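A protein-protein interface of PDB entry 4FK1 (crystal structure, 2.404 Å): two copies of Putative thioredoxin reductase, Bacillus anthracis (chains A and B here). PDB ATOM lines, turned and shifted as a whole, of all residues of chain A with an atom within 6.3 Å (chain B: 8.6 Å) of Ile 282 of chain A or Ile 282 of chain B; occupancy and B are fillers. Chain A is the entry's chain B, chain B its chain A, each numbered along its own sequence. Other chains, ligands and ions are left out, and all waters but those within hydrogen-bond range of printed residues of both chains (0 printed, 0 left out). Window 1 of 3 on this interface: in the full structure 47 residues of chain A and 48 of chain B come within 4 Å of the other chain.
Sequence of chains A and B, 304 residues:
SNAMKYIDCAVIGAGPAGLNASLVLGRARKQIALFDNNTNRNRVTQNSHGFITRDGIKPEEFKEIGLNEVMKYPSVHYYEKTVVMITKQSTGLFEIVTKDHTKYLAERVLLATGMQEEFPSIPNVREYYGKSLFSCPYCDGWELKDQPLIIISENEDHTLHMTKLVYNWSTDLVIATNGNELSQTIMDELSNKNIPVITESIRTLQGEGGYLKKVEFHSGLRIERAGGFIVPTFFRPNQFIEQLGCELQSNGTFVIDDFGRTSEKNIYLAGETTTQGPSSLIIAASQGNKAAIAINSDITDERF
Of the 14 printed residues of chain A, 9 touch a printed residue of chain B. Printed residues of chain B that touch a printed residue of chain A: Asn 20, Leu 23, Gly 50, Phe 51, Ile 52, Ser 280, Ile 282, Ile 283, Ala 285, Ser 286, Asn 289 and Lys 290. Hydrophobic or aromatic side chains of chain B within 4 Å of the printed part of chain A: Leu 23, Phe 51, Ile 52, Ile 282 and Ala 285. Among the printed residues, 25 pairs touch across the chains.
Asn 20 of chain A touches Gly 50 of chain B, and with the chains exchanged Gly 50 of chain A touches Asn 20 of chain B. Phe 51 of chain A touches its own counterpart, Phe 51 of chain B. Ile 282 of chain A touches its own counterpart, Ile 282 of chain B. Positions printed for both chains: 16, 20, 50, 51, 52, 280, 281, 282, 283, 284, 285, 286, 287 and 289.
Among the printed residues, merely in contact across the chains: Asn 289 of chain A with Ile 282 of chain B, Ile 282 of chain A with Asn 289 of chain B, Ile 283 of chain A with Ser 286 of chain B, Ile 282 of chain A with Asn 20 of chain B, Ser 286 of chain A with Ile 282 of chain B, Ile 283 of chain A with Lys 290 of chain B, Phe 51 of chain A with Phe 51 of chain B, Ile 282 of chain A with Ile 282 of chain B, Asn 20 of chain A with Ile 282 of chain B, Gly 50 of chain A with Leu 23 of chain B, Ile 282 of chain A with Ala 285 of chain B, Phe 51 of chain A with Ile 52 of chain B, Ile 282 of chain A with Ser 286 of chain B, Ile 52 of chain A with Phe 51 of chain B, Ser 286 of chain A with Ile 283 of chain B, Ile 282 of chain A with Phe 51 of chain B, Ile 52 of chain A with Ala 285 of chain B and Ile 283 of chain A with Asn 289 of chain B.
Pro 16 of chain A touches none of the printed residues of chain B. Printed residues of chain B within 4 Å of Phe 51 of chain A: Phe 51 and Ile 52. Ile 282 of chain A touches six residues of chain B. Printed residues of chain A within 4 Å of Asn 20 of chain B: Gly 50 (2.7 Å), Ile 52 (3.2 Å) and Ile 282 (3.5 Å). Of the printed residues of chain A, Ile 282 of chain B touches Asn 20, Ile 282, Ser 286 and Asn 289. Printed residues of chain A within 4 Å of Asn 289 of chain B: Ser 280, Ile 282 and Ile 283. The nearest residue of chain B that does not touch Ile 282 of chain A is Leu 281 of chain B (6.2 Å). The nearest printed residue of chain A that does not touch Ile 282 of chain B is Ala 285 of chain A (4.001 Å).
The backbone carbonyl oxygen (O) of Gly 50 of chain A sits at hydrogen-bond distance from the side-chain amide nitrogen (ND2) of Asn 20 of chain B. OD1 of Asn 20 of chain B lies close to N of Ile 52 of chain A (3.3 Å). ND2 of Asn 20 of chain A is in hydrogen-bond range of O of Gly 50 of chain B (2.9 Å). The backbone NH (N) of Ile 52 of chain B sits close to the side-chain amide oxygen (OD1) of Asn 20 of chain A, at 3.2 Å. The side-chain amide oxygen (OD1) of Asn 289 of chain A lies within hydrogen-bond range of the side-chain hydroxyl (OG) of Ser 280 of chain B (2.9 Å). The side-chain hydroxyl (OG) of Ser 286 of chain A lies within hydrogen-bond range of the side-chain hydroxyl (OG) of Ser 286 of chain B (3.1 Å). OD1 of Asn 289 of chain B is in hydrogen-bond range of OG of Ser 280 of chain A (2.9 Å).
The backbone NH (N) of Ile 282 of chain B lies close to the side-chain hydroxyl (OG) of Ser 280 of chain B, at 3.5 Å. The backbone NH (N) of Ile 283 of chain B sits close to the side-chain hydroxyl (OG) of Ser 280 of chain B (3.4 Å). N of Ile 283 of chain A sits close to OG of Ser 280 of chain A, at 3.3 Å. O of Ile 283 of chain A is in hydrogen-bond range of OG of Ser 286 of chain A (3.0 Å).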
ATOM      1  N   PRO A  16     -25.453 -32.913 -19.474  1.00  0.00           N
ATOM      2  CA  PRO A  16     -24.715 -31.692 -19.134  1.00  0.00           C
ATOM      3  C   PRO A  16     -25.495 -30.842 -18.148  1.00  0.00           C
ATOM      4  O   PRO A  16     -24.887 -30.206 -17.282  1.00  0.00           O
ATOM      5  CB  PRO A  16     -24.591 -30.978 -20.470  1.00  0.00           C
ATOM      6  CG  PRO A  16     -24.689 -32.089 -21.492  1.00  0.00           C
ATOM      7  CD  PRO A  16     -25.644 -33.065 -20.928  1.00  0.00           C
ATOM      8  N   ASN A  20     -23.896 -30.030 -14.464  1.00  0.00           N
ATOM      9  CA  ASN A  20     -23.564 -28.671 -14.086  1.00  0.00           C
ATOM     10  C   ASN A  20     -24.409 -28.187 -12.915  1.00  0.00           C
ATOM     11  O   ASN A  20     -23.981 -27.333 -12.139  1.00  0.00           O
ATOM     12  CB  ASN A  20     -23.724 -27.732 -15.274  1.00  0.00           C
ATOM     13  CG  ASN A  20     -22.701 -26.623 -15.268  1.00  0.00           C
ATOM     14  OD1 ASN A  20     -21.907 -26.500 -16.201  1.00  0.00           O
ATOM     15  ND2 ASN A  20     -22.696 -25.819 -14.206  1.00  0.00           N
ATOM     16  N   GLY A  50     -18.966 -27.730 -30.518  1.00  0.00           N
ATOM     17  CA  GLY A  50     -19.696 -26.516 -30.184  1.00  0.00           C
ATOM     18  C   GLY A  50     -19.644 -26.108 -28.727  1.00  0.00           C
ATOM     19  O   GLY A  50     -20.057 -25.001 -28.371  1.00  0.00           O
ATOM     20  N   PHE A  51     -19.158 -27.022 -27.886  1.00  0.00           N
ATOM     21  CA  PHE A  51     -18.948 -26.775 -26.464  1.00  0.00           C
ATOM     22  C   PHE A  51     -17.528 -26.252 -26.333  1.00  0.00           C
ATOM     23  O   PHE A  51     -16.568 -26.988 -26.564  1.00  0.00           O
ATOM     24  CB  PHE A  51     -19.108 -28.090 -25.697  1.00  0.00           C
ATOM     25  CG  PHE A  51     -19.176 -27.941 -24.189  1.00  0.00           C
ATOM     26  CD1 PHE A  51     -18.039 -27.686 -23.446  1.00  0.00           C
ATOM     27  CD2 PHE A  51     -20.382 -28.107 -23.521  1.00  0.00           C
ATOM     28  CE1 PHE A  51     -18.104 -27.580 -22.058  1.00  0.00           C
ATOM     29  CE2 PHE A  51     -20.459 -28.005 -22.142  1.00  0.00           C
ATOM     30  CZ  PHE A  51     -19.313 -27.737 -21.405  1.00  0.00           C
ATOM     31  N   ILE A  52     -17.385 -24.978 -25.981  1.00  0.00           N
ATOM     32  CA  ILE A  52     -16.056 -24.348 -25.886  1.00  0.00           C
ATOM     33  C   ILE A  52     -15.107 -25.067 -24.906  1.00  0.00           C
ATOM     34  O   ILE A  52     -15.513 -25.440 -23.805  1.00  0.00           O
ATOM     35  CB  ILE A  52     -16.157 -22.805 -25.594  1.00  0.00           C
ATOM     36  CG1 ILE A  52     -14.825 -22.127 -25.857  1.00  0.00           C
ATOM     37  CG2 ILE A  52     -16.661 -22.514 -24.209  1.00  0.00           C
ATOM     38  CD1 ILE A  52     -14.400 -22.251 -27.291  1.00  0.00           C
ATOM     39  N   SER A 280     -28.245 -27.599 -27.057  1.00  0.00           N
ATOM     40  CA  SER A 280     -26.850 -27.989 -27.219  1.00  0.00           C
ATOM     41  C   SER A 280     -26.253 -28.422 -25.875  1.00  0.00           C
ATOM     42  O   SER A 280     -26.891 -28.271 -24.839  1.00  0.00           O
ATOM     43  CB  SER A 280     -26.040 -26.839 -27.839  1.00  0.00           C
ATOM     44  OG  SER A 280     -26.171 -25.647 -27.072  1.00  0.00           O
ATOM     45  N   LEU A 281     -25.046 -28.975 -25.901  1.00  0.00           N
ATOM     46  CA  LEU A 281     -24.366 -29.342 -24.674  1.00  0.00           C
ATOM     47  C   LEU A 281     -24.191 -28.114 -23.777  1.00  0.00           C
ATOM     48  O   LEU A 281     -24.581 -28.134 -22.612  1.00  0.00           O
ATOM     49  CB  LEU A 281     -23.004 -29.960 -24.979  1.00  0.00           C
ATOM     50  CG  LEU A 281     -22.969 -31.356 -25.605  1.00  0.00           C
ATOM     51  CD1 LEU A 281     -21.538 -31.795 -25.817  1.00  0.00           C
ATOM     52  CD2 LEU A 281     -23.684 -32.363 -24.740  1.00  0.00           C
ATOM     53  N   ILE A 282     -23.633 -27.046 -24.346  1.00  0.00           N
ATOM     54  CA  ILE A 282     -23.291 -25.838 -23.611  1.00  0.00           C
ATOM     55  C   ILE A 282     -24.528 -25.094 -23.082  1.00  0.00           C
ATOM     56  O   ILE A 282     -24.486 -24.501 -22.004  1.00  0.00           O
ATOM     57  CB  ILE A 282     -22.375 -24.890 -24.452  1.00  0.00           C
ATOM     58  CG1 ILE A 282     -21.587 -23.940 -23.546  1.00  0.00           C
ATOM     59  CG2 ILE A 282     -23.173 -24.088 -25.471  1.00  0.00           C
ATOM     60  CD1 ILE A 282     -20.447 -24.611 -22.809  1.00  0.00           C
ATOM     61  N   ILE A 283     -25.634 -25.161 -23.816  1.00  0.00           N
ATOM     62  CA  ILE A 283     -26.857 -24.470 -23.428  1.00  0.00           C
ATOM     63  C   ILE A 283     -27.579 -25.212 -22.304  1.00  0.00           C
ATOM     64  O   ILE A 283     -28.052 -24.595 -21.354  1.00  0.00           O
ATOM     65  CB  ILE A 283     -27.799 -24.259 -24.635  1.00  0.00           C
ATOM     66  CG1 ILE A 283     -27.304 -23.089 -25.490  1.00  0.00           C
ATOM     67  CG2 ILE A 283     -29.229 -24.002 -24.181  1.00  0.00           C
ATOM     68  CD1 ILE A 283     -28.018 -22.961 -26.849  1.00  0.00           C
ATOM     69  N   ALA A 284     -27.657 -26.531 -22.413  1.00  0.00           N
ATOM     70  CA  ALA A 284     -28.227 -27.340 -21.348  1.00  0.00           C
ATOM     71  C   ALA A 284     -27.419 -27.151 -20.053  1.00  0.00           C
ATOM     72  O   ALA A 284     -27.970 -26.816 -18.999  1.00  0.00           O
ATOM     73  CB  ALA A 284     -28.257 -28.798 -21.754  1.00  0.00           C
ATOM     74  N   ALA A 285     -26.108 -27.350 -20.162  1.00  0.00           N
ATOM     75  CA  ALA A 285     -25.184 -27.151 -19.062  1.00  0.00           C
ATOM     76  C   ALA A 285     -25.441 -25.837 -18.319  1.00  0.00           C
ATOM     77  O   ALA A 285     -25.432 -25.812 -17.092  1.00  0.00           O
ATOM     78  CB  ALA A 285     -23.757 -27.212 -19.575  1.00  0.00           C
ATOM     79  N   SER A 286     -25.695 -24.756 -19.054  1.00  0.00           N
ATOM     80  CA  SER A 286     -25.918 -23.453 -18.422  1.00  0.00           C
ATOM     81  C   SER A 286     -27.300 -23.398 -17.791  1.00  0.00           C
ATOM     82  O   SER A 286     -27.522 -22.668 -16.820  1.00  0.00           O
ATOM     83  CB  SER A 286     -25.758 -22.298 -19.409  1.00  0.00           C
ATOM     84  OG  SER A 286     -26.963 -22.069 -20.118  1.00  0.00           O
ATOM     85  N   GLN A 287     -28.233 -24.171 -18.341  1.00  0.00           N
ATOM     86  CA  GLN A 287     -29.549 -24.290 -17.727  1.00  0.00           C
ATOM     87  C   GLN A 287     -29.489 -25.100 -16.418  1.00  0.00           C
ATOM     88  O   GLN A 287     -30.428 -25.083 -15.625  1.00  0.00           O
ATOM     89  CB  GLN A 287     -30.538 -24.919 -18.703  1.00  0.00           C
ATOM     90  CG  GLN A 287     -31.013 -23.951 -19.782  1.00  0.00           C
ATOM     91  CD  GLN A 287     -31.729 -24.633 -20.939  1.00  0.00           C
ATOM     92  OE1 GLN A 287     -32.158 -25.783 -20.843  1.00  0.00           O
ATOM     93  NE2 GLN A 287     -31.851 -23.919 -22.050  1.00  0.00           N
ATOM     94  N   ASN A 289     -26.686 -24.849 -14.276  1.00  0.00           N
ATOM     95  CA  ASN A 289     -26.225 -23.718 -13.502  1.00  0.00           C
ATOM     96  C   ASN A 289     -27.384 -22.829 -13.031  1.00  0.00           C
ATOM     97  O   ASN A 289     -27.533 -22.594 -11.825  1.00  0.00           O
ATOM     98  CB  ASN A 289     -25.224 -22.908 -14.332  1.00  0.00           C
ATOM     99  CG  ASN A 289     -24.392 -21.952 -13.495  1.00  0.00           C
ATOM    100  OD1 ASN A 289     -23.300 -21.562 -13.889  1.00  0.00           O
ATOM    101  ND2 ASN A 289     -24.899 -21.581 -12.328  1.00  0.00           N
ATOM    102  N   PRO B  16     -15.594 -16.386 -22.637  1.00  0.00           N
ATOM    103  CA  PRO B  16     -16.421 -17.555 -22.965  1.00  0.00           C
ATOM    104  C   PRO B  16     -17.495 -17.229 -24.004  1.00  0.00           C
ATOM    105  O   PRO B  16     -17.771 -18.062 -24.873  1.00  0.00           O
ATOM    106  CB  PRO B  16     -17.064 -17.926 -21.620  1.00  0.00           C
ATOM    107  CG  PRO B  16     -16.780 -16.756 -20.692  1.00  0.00           C
ATOM    108  CD  PRO B  16     -15.510 -16.152 -21.186  1.00  0.00           C
ATOM    109  N   ALA B  17     -18.072 -16.032 -23.923  1.00  0.00           N
ATOM    110  CA  ALA B  17     -19.123 -15.636 -24.847  1.00  0.00           C
ATOM    111  C   ALA B  17     -18.630 -15.539 -26.307  1.00  0.00           C
ATOM    112  O   ALA B  17     -19.119 -16.263 -27.186  1.00  0.00           O
ATOM    113  CB  ALA B  17     -19.750 -14.339 -24.402  1.00  0.00           C
ATOM    114  N   ASN B  20     -17.280 -18.937 -27.778  1.00  0.00           N
ATOM    115  CA  ASN B  20     -18.226 -19.993 -28.104  1.00  0.00           C
ATOM    116  C   ASN B  20     -19.081 -19.574 -29.305  1.00  0.00           C
ATOM    117  O   ASN B  20     -19.507 -20.407 -30.110  1.00  0.00           O
ATOM    118  CB  ASN B  20     -19.098 -20.319 -26.895  1.00  0.00           C
ATOM    119  CG  ASN B  20     -19.530 -21.768 -26.867  1.00  0.00           C
ATOM    120  OD1 ASN B  20     -19.446 -22.421 -25.831  1.00  0.00           O
ATOM    121  ND2 ASN B  20     -19.998 -22.280 -28.006  1.00  0.00           N
ATOM    122  N   ALA B  21     -19.324 -18.269 -29.408  1.00  0.00           N
ATOM    123  CA  ALA B  21     -19.979 -17.687 -30.563  1.00  0.00           C
ATOM    124  C   ALA B  21     -19.103 -17.875 -31.796  1.00  0.00           C
ATOM    125  O   ALA B  21     -19.581 -18.275 -32.849  1.00  0.00           O
ATOM    126  CB  ALA B  21     -20.248 -16.215 -30.322  1.00  0.00           C
ATOM    127  N   LEU B  23     -16.831 -20.144 -32.247  1.00  0.00           N
ATOM    128  CA  LEU B  23     -16.761 -21.581 -32.532  1.00  0.00           C
ATOM    129  C   LEU B  23     -17.924 -22.064 -33.403  1.00  0.00           C
ATOM    130  O   LEU B  23     -17.719 -22.751 -34.412  1.00  0.00           O
ATOM    131  CB  LEU B  23     -16.732 -22.387 -31.235  1.00  0.00           C
ATOM    132  CG  LEU B  23     -16.680 -23.909 -31.368  1.00  0.00           C
ATOM    133  CD1 LEU B  23     -15.508 -24.314 -32.236  1.00  0.00           C
ATOM    134  CD2 LEU B  23     -16.588 -24.575 -29.988  1.00  0.00           C
ATOM    135  N   VAL B  24     -19.141 -21.703 -33.004  1.00  0.00           N
ATOM    136  CA  VAL B  24     -20.340 -22.089 -33.740  1.00  0.00           C
ATOM    137  C   VAL B  24     -20.403 -21.413 -35.124  1.00  0.00           C
ATOM    138  O   VAL B  24     -20.812 -22.024 -36.111  1.00  0.00           O
ATOM    139  CB  VAL B  24     -21.610 -21.752 -32.924  1.00  0.00           C
ATOM    140  CG1 VAL B  24     -22.849 -22.152 -33.691  1.00  0.00           C
ATOM    141  CG2 VAL B  24     -21.570 -22.471 -31.566  1.00  0.00           C
ATOM    142  N   HIS B  49     -14.336 -22.198 -11.100  1.00  0.00           N
ATOM    143  CA  HIS B  49     -15.111 -23.410 -10.869  1.00  0.00           C
ATOM    144  C   HIS B  49     -16.542 -23.245 -11.387  1.00  0.00           C
ATOM    145  O   HIS B  49     -17.000 -22.124 -11.612  1.00  0.00           O
ATOM    146  CB  HIS B  49     -15.139 -23.753  -9.375  1.00  0.00           C
ATOM    147  CG  HIS B  49     -13.784 -23.788  -8.728  1.00  0.00           C
ATOM    148  ND1 HIS B  49     -13.172 -24.960  -8.337  1.00  0.00           N
ATOM    149  CD2 HIS B  49     -12.938 -22.788  -8.378  1.00  0.00           C
ATOM    150  CE1 HIS B  49     -12.000 -24.684  -7.790  1.00  0.00           C
ATOM    151  NE2 HIS B  49     -11.831 -23.374  -7.811  1.00  0.00           N
ATOM    152  N   GLY B  50     -17.256 -24.352 -11.577  1.00  0.00           N
ATOM    153  CA  GLY B  50     -18.665 -24.266 -11.940  1.00  0.00           C
ATOM    154  C   GLY B  50     -18.967 -24.455 -13.419  1.00  0.00           C
ATOM    155  O   GLY B  50     -20.116 -24.623 -13.821  1.00  0.00           O
ATOM    156  N   PHE B  51     -17.914 -24.410 -14.225  1.00  0.00           N
ATOM    157  CA  PHE B  51     -17.968 -24.767 -15.628  1.00  0.00           C
ATOM    158  C   PHE B  51     -17.708 -26.262 -15.729  1.00  0.00           C
ATOM    159  O   PHE B  51     -16.561 -26.689 -15.650  1.00  0.00           O
ATOM    160  CB  PHE B  51     -16.863 -24.021 -16.364  1.00  0.00           C
ATOM    161  CG  PHE B  51     -16.994 -24.039 -17.860  1.00  0.00           C
ATOM    162  CD1 PHE B  51     -17.524 -22.947 -18.533  1.00  0.00           C
ATOM    163  CD2 PHE B  51     -16.564 -25.134 -18.601  1.00  0.00           C
ATOM    164  CE1 PHE B  51     -17.632 -22.944 -19.916  1.00  0.00           C
ATOM    165  CE2 PHE B  51     -16.671 -25.139 -19.985  1.00  0.00           C
ATOM    166  CZ  PHE B  51     -17.206 -24.040 -20.643  1.00  0.00           C
ATOM    167  N   ILE B  52     -18.767 -27.054 -15.920  1.00  0.00           N
ATOM    168  CA  ILE B  52     -18.657 -28.519 -16.013  1.00  0.00           C
ATOM    169  C   ILE B  52     -17.595 -29.023 -17.011  1.00  0.00           C
ATOM    170  O   ILE B  52     -17.517 -28.549 -18.157  1.00  0.00           O
ATOM    171  CB  ILE B  52     -20.037 -29.192 -16.289  1.00  0.00           C
ATOM    172  CG1 ILE B  52     -19.955 -30.693 -16.035  1.00  0.00           C
ATOM    173  CG2 ILE B  52     -20.536 -28.892 -17.701  1.00  0.00           C
ATOM    174  CD1 ILE B  52     -19.474 -31.030 -14.631  1.00  0.00           C
ATOM    175  N   THR B  53     -16.792 -29.984 -16.539  1.00  0.00           N
ATOM    176  CA  THR B  53     -15.609 -30.555 -17.218  1.00  0.00           C
ATOM    177  C   THR B  53     -14.371 -29.646 -17.173  1.00  0.00           C
ATOM    178  O   THR B  53     -13.283 -30.051 -17.585  1.00  0.00           O
ATOM    179  CB  THR B  53     -15.872 -31.046 -18.679  1.00  0.00           C
ATOM    180  OG1 THR B  53     -15.772 -29.945 -19.591  1.00  0.00           O
ATOM    181  CG2 THR B  53     -17.238 -31.735 -18.806  1.00  0.00           C
ATOM    182  N   ARG B  54     -14.542 -28.423 -16.674  1.00  0.00           N
ATOM    183  CA  ARG B  54     -13.426 -27.493 -16.472  1.00  0.00           C
ATOM    184  C   ARG B  54     -13.383 -26.965 -15.017  1.00  0.00           C
ATOM    185  O   ARG B  54     -12.753 -25.946 -14.728  1.00  0.00           O
ATOM    186  CB  ARG B  54     -13.500 -26.337 -17.486  1.00  0.00           C
ATOM    187  CG  ARG B  54     -13.333 -26.743 -18.987  1.00  0.00           C
ATOM    188  CD  ARG B  54     -11.959 -27.361 -19.194  1.00  0.00           C
ATOM    189  NE  ARG B  54     -11.664 -27.742 -20.565  1.00  0.00           N
ATOM    190  CZ  ARG B  54     -10.547 -28.368 -20.921  1.00  0.00           C
ATOM    191  NH1 ARG B  54     -10.318 -28.690 -22.189  1.00  0.00           N
ATOM    192  NH2 ARG B  54      -9.655 -28.677 -19.997  1.00  0.00           N
ATOM    193  N   PHE B  62      -8.162 -21.531 -19.675  1.00  0.00           N
ATOM    194  CA  PHE B  62      -9.470 -21.623 -20.328  1.00  0.00           C
ATOM    195  C   PHE B  62      -9.472 -20.826 -21.629  1.00  0.00           C
ATOM    196  O   PHE B  62      -9.737 -21.362 -22.698  1.00  0.00           O
ATOM    197  CB  PHE B  62     -10.542 -21.081 -19.384  1.00  0.00           C
ATOM    198  CG  PHE B  62     -11.947 -21.279 -19.869  1.00  0.00           C
ATOM    199  CD1 PHE B  62     -12.676 -22.385 -19.479  1.00  0.00           C
ATOM    200  CD2 PHE B  62     -12.552 -20.337 -20.687  1.00  0.00           C
ATOM    201  CE1 PHE B  62     -13.979 -22.560 -19.918  1.00  0.00           C
ATOM    202  CE2 PHE B  62     -13.845 -20.505 -21.132  1.00  0.00           C
ATOM    203  CZ  PHE B  62     -14.563 -21.620 -20.745  1.00  0.00           C
ATOM    204  N   SER B 279     -22.558 -13.191 -14.224  1.00  0.00           N
ATOM    205  CA  SER B 279     -23.139 -14.528 -14.361  1.00  0.00           C
ATOM    206  C   SER B 279     -22.132 -15.622 -14.016  1.00  0.00           C
ATOM    207  O   SER B 279     -21.854 -15.878 -12.836  1.00  0.00           O
ATOM    208  CB  SER B 279     -23.731 -14.747 -15.767  1.00  0.00           C
ATOM    209  OG  SER B 279     -22.803 -14.455 -16.805  1.00  0.00           O
ATOM    210  N   SER B 280     -21.603 -16.269 -15.049  1.00  0.00           N
ATOM    211  CA  SER B 280     -20.583 -17.312 -14.912  1.00  0.00           C
ATOM    212  C   SER B 280     -20.043 -17.648 -16.303  1.00  0.00           C
ATOM    213  O   SER B 280     -20.612 -17.196 -17.317  1.00  0.00           O
ATOM    214  CB  SER B 280     -21.160 -18.579 -14.254  1.00  0.00           C
ATOM    215  OG  SER B 280     -21.913 -19.337 -15.201  1.00  0.00           O
ATOM    216  N   LEU B 281     -18.971 -18.435 -16.357  1.00  0.00           N
ATOM    217  CA  LEU B 281     -18.380 -18.831 -17.623  1.00  0.00           C
ATOM    218  C   LEU B 281     -19.367 -19.621 -18.491  1.00  0.00           C
ATOM    219  O   LEU B 281     -19.505 -19.379 -19.697  1.00  0.00           O
ATOM    220  CB  LEU B 281     -17.130 -19.662 -17.382  1.00  0.00           C
ATOM    221  CG  LEU B 281     -16.040 -18.989 -16.544  1.00  0.00           C
ATOM    222  CD1 LEU B 281     -14.948 -19.987 -16.176  1.00  0.00           C
ATOM    223  CD2 LEU B 281     -15.460 -17.794 -17.271  1.00  0.00           C
ATOM    224  N   ILE B 282     -20.057 -20.565 -17.861  1.00  0.00           N
ATOM    225  CA  ILE B 282     -20.929 -21.472 -18.590  1.00  0.00           C
ATOM    226  C   ILE B 282     -22.150 -20.743 -19.166  1.00  0.00           C
ATOM    227  O   ILE B 282     -22.594 -21.067 -20.257  1.00  0.00           O
ATOM    228  CB  ILE B 282     -21.326 -22.718 -17.737  1.00  0.00           C
ATOM    229  CG1 ILE B 282     -21.763 -23.873 -18.635  1.00  0.00           C
ATOM    230  CG2 ILE B 282     -22.414 -22.393 -16.749  1.00  0.00           C
ATOM    231  CD1 ILE B 282     -20.619 -24.618 -19.256  1.00  0.00           C
ATOM    232  N   ILE B 283     -22.658 -19.742 -18.447  1.00  0.00           N
ATOM    233  CA  ILE B 283     -23.797 -18.950 -18.907  1.00  0.00           C
ATOM    234  C   ILE B 283     -23.394 -18.069 -20.097  1.00  0.00           C
ATOM    235  O   ILE B 283     -24.020 -18.121 -21.164  1.00  0.00           O
ATOM    236  CB  ILE B 283     -24.413 -18.115 -17.759  1.00  0.00           C
ATOM    237  CG1 ILE B 283     -24.909 -19.047 -16.652  1.00  0.00           C
ATOM    238  CG2 ILE B 283     -25.576 -17.269 -18.266  1.00  0.00           C
ATOM    239  CD1 ILE B 283     -25.620 -18.343 -15.514  1.00  0.00           C
ATOM    240  N   ALA B 284     -22.323 -17.302 -19.918  1.00  0.00           N
ATOM    241  CA  ALA B 284     -21.707 -16.538 -21.001  1.00  0.00           C
ATOM    242  C   ALA B 284     -21.450 -17.363 -22.271  1.00  0.00           C
ATOM    243  O   ALA B 284     -21.708 -16.889 -23.369  1.00  0.00           O
ATOM    244  CB  ALA B 284     -20.414 -15.919 -20.528  1.00  0.00           C
ATOM    245  N   ALA B 285     -20.911 -18.572 -22.116  1.00  0.00           N
ATOM    246  CA  ALA B 285     -20.636 -19.433 -23.259  1.00  0.00           C
ATOM    247  C   ALA B 285     -21.935 -19.762 -23.985  1.00  0.00           C
ATOM    248  O   ALA B 285     -22.010 -19.755 -25.220  1.00  0.00           O
ATOM    249  CB  ALA B 285     -19.938 -20.727 -22.807  1.00  0.00           C
ATOM    250  N   SER B 286     -22.954 -20.059 -23.189  1.00  0.00           N
ATOM    251  CA  SER B 286     -24.262 -20.412 -23.691  1.00  0.00           C
ATOM    252  C   SER B 286     -24.835 -19.227 -24.474  1.00  0.00           C
ATOM    253  O   SER B 286     -25.420 -19.399 -25.539  1.00  0.00           O
ATOM    254  CB  SER B 286     -25.167 -20.781 -22.519  1.00  0.00           C
ATOM    255  OG  SER B 286     -26.493 -20.996 -22.949  1.00  0.00           O
ATOM    256  N   GLN B 287     -24.652 -18.020 -23.953  1.00  0.00           N
ATOM    257  CA  GLN B 287     -25.161 -16.836 -24.628  1.00  0.00           C
ATOM    258  C   GLN B 287     -24.403 -16.546 -25.930  1.00  0.00           C
ATOM    259  O   GLN B 287     -24.965 -15.982 -26.869  1.00  0.00           O
ATOM    260  CB  GLN B 287     -25.140 -15.632 -23.690  1.00  0.00           C
ATOM    261  CG  GLN B 287     -26.240 -15.643 -22.645  1.00  0.00           C
ATOM    262  CD  GLN B 287     -26.029 -14.561 -21.596  1.00  0.00           C
ATOM    263  OE1 GLN B 287     -25.084 -13.781 -21.685  1.00  0.00           O
ATOM    264  NE2 GLN B 287     -26.909 -14.507 -20.607  1.00  0.00           N
ATOM    265  N   GLY B 288     -23.130 -16.934 -25.967  1.00  0.00           N
ATOM    266  CA  GLY B 288     -22.353 -16.932 -27.186  1.00  0.00           C
ATOM    267  C   GLY B 288     -22.956 -17.892 -28.218  1.00  0.00           C
ATOM    268  O   GLY B 288     -23.207 -17.498 -29.363  1.00  0.00           O
ATOM    269  N   ASN B 289     -23.181 -19.146 -27.813  1.00  0.00           N
ATOM    270  CA  ASN B 289     -23.838 -20.135 -28.669  1.00  0.00           C
ATOM    271  C   ASN B 289     -25.168 -19.565 -29.204  1.00  0.00           C
ATOM    272  O   ASN B 289     -25.444 -19.633 -30.414  1.00  0.00           O
ATOM    273  CB  ASN B 289     -24.045 -21.471 -27.916  1.00  0.00           C
ATOM    274  CG  ASN B 289     -24.475 -22.643 -28.836  1.00  0.00           C
ATOM    275  OD1 ASN B 289     -24.452 -23.810 -28.427  1.00  0.00           O
ATOM    276  ND2 ASN B 289     -24.836 -22.340 -30.071  1.00  0.00           N
ATOM    277  N   LYS B 290     -25.976 -18.988 -28.321  1.00  0.00           N
ATOM    278  CA  LYS B 290     -27.252 -18.420 -28.734  1.00  0.00           C
ATOM    279  C   LYS B 290     -27.113 -17.311 -29.810  1.00  0.00           C
ATOM    280  O   LYS B 290     -27.838 -17.305 -30.823  1.00  0.00           O
ATOM    281  CB  LYS B 290     -28.014 -17.904 -27.522  1.00  0.00           C
ATOM    282  CG  LYS B 290     -29.312 -18.621 -27.236  1.00  0.00           C
ATOM    283  CD  LYS B 290     -29.139 -19.710 -26.187  1.00  0.00           C
ATOM    284  CE  LYS B 290     -29.083 -19.151 -24.782  1.00  0.00           C
ATOM    285  NZ  LYS B 290     -30.430 -18.794 -24.258  1.00  0.00           N
ATOM    286  N   ILE B 293     -26.335 -18.563 -33.195  1.00  0.00           N
ATOM    287  CA  ILE B 293     -27.509 -19.092 -33.868  1.00  0.00           C
ATOM    288  C   ILE B 293     -28.367 -17.991 -34.494  1.00  0.00           C
ATOM    289  O   ILE B 293     -28.925 -18.185 -35.568  1.00  0.00           O
ATOM    290  CB  ILE B 293     -28.325 -19.987 -32.954  1.00  0.00           C
ATOM    291  CG1 ILE B 293     -27.467 -21.190 -32.571  1.00  0.00           C
ATOM    292  CG2 ILE B 293     -29.597 -20.461 -33.661  1.00  0.00           C
ATOM    293  CD1 ILE B 293     -28.224 -22.262 -31.888  1.00  0.00           C
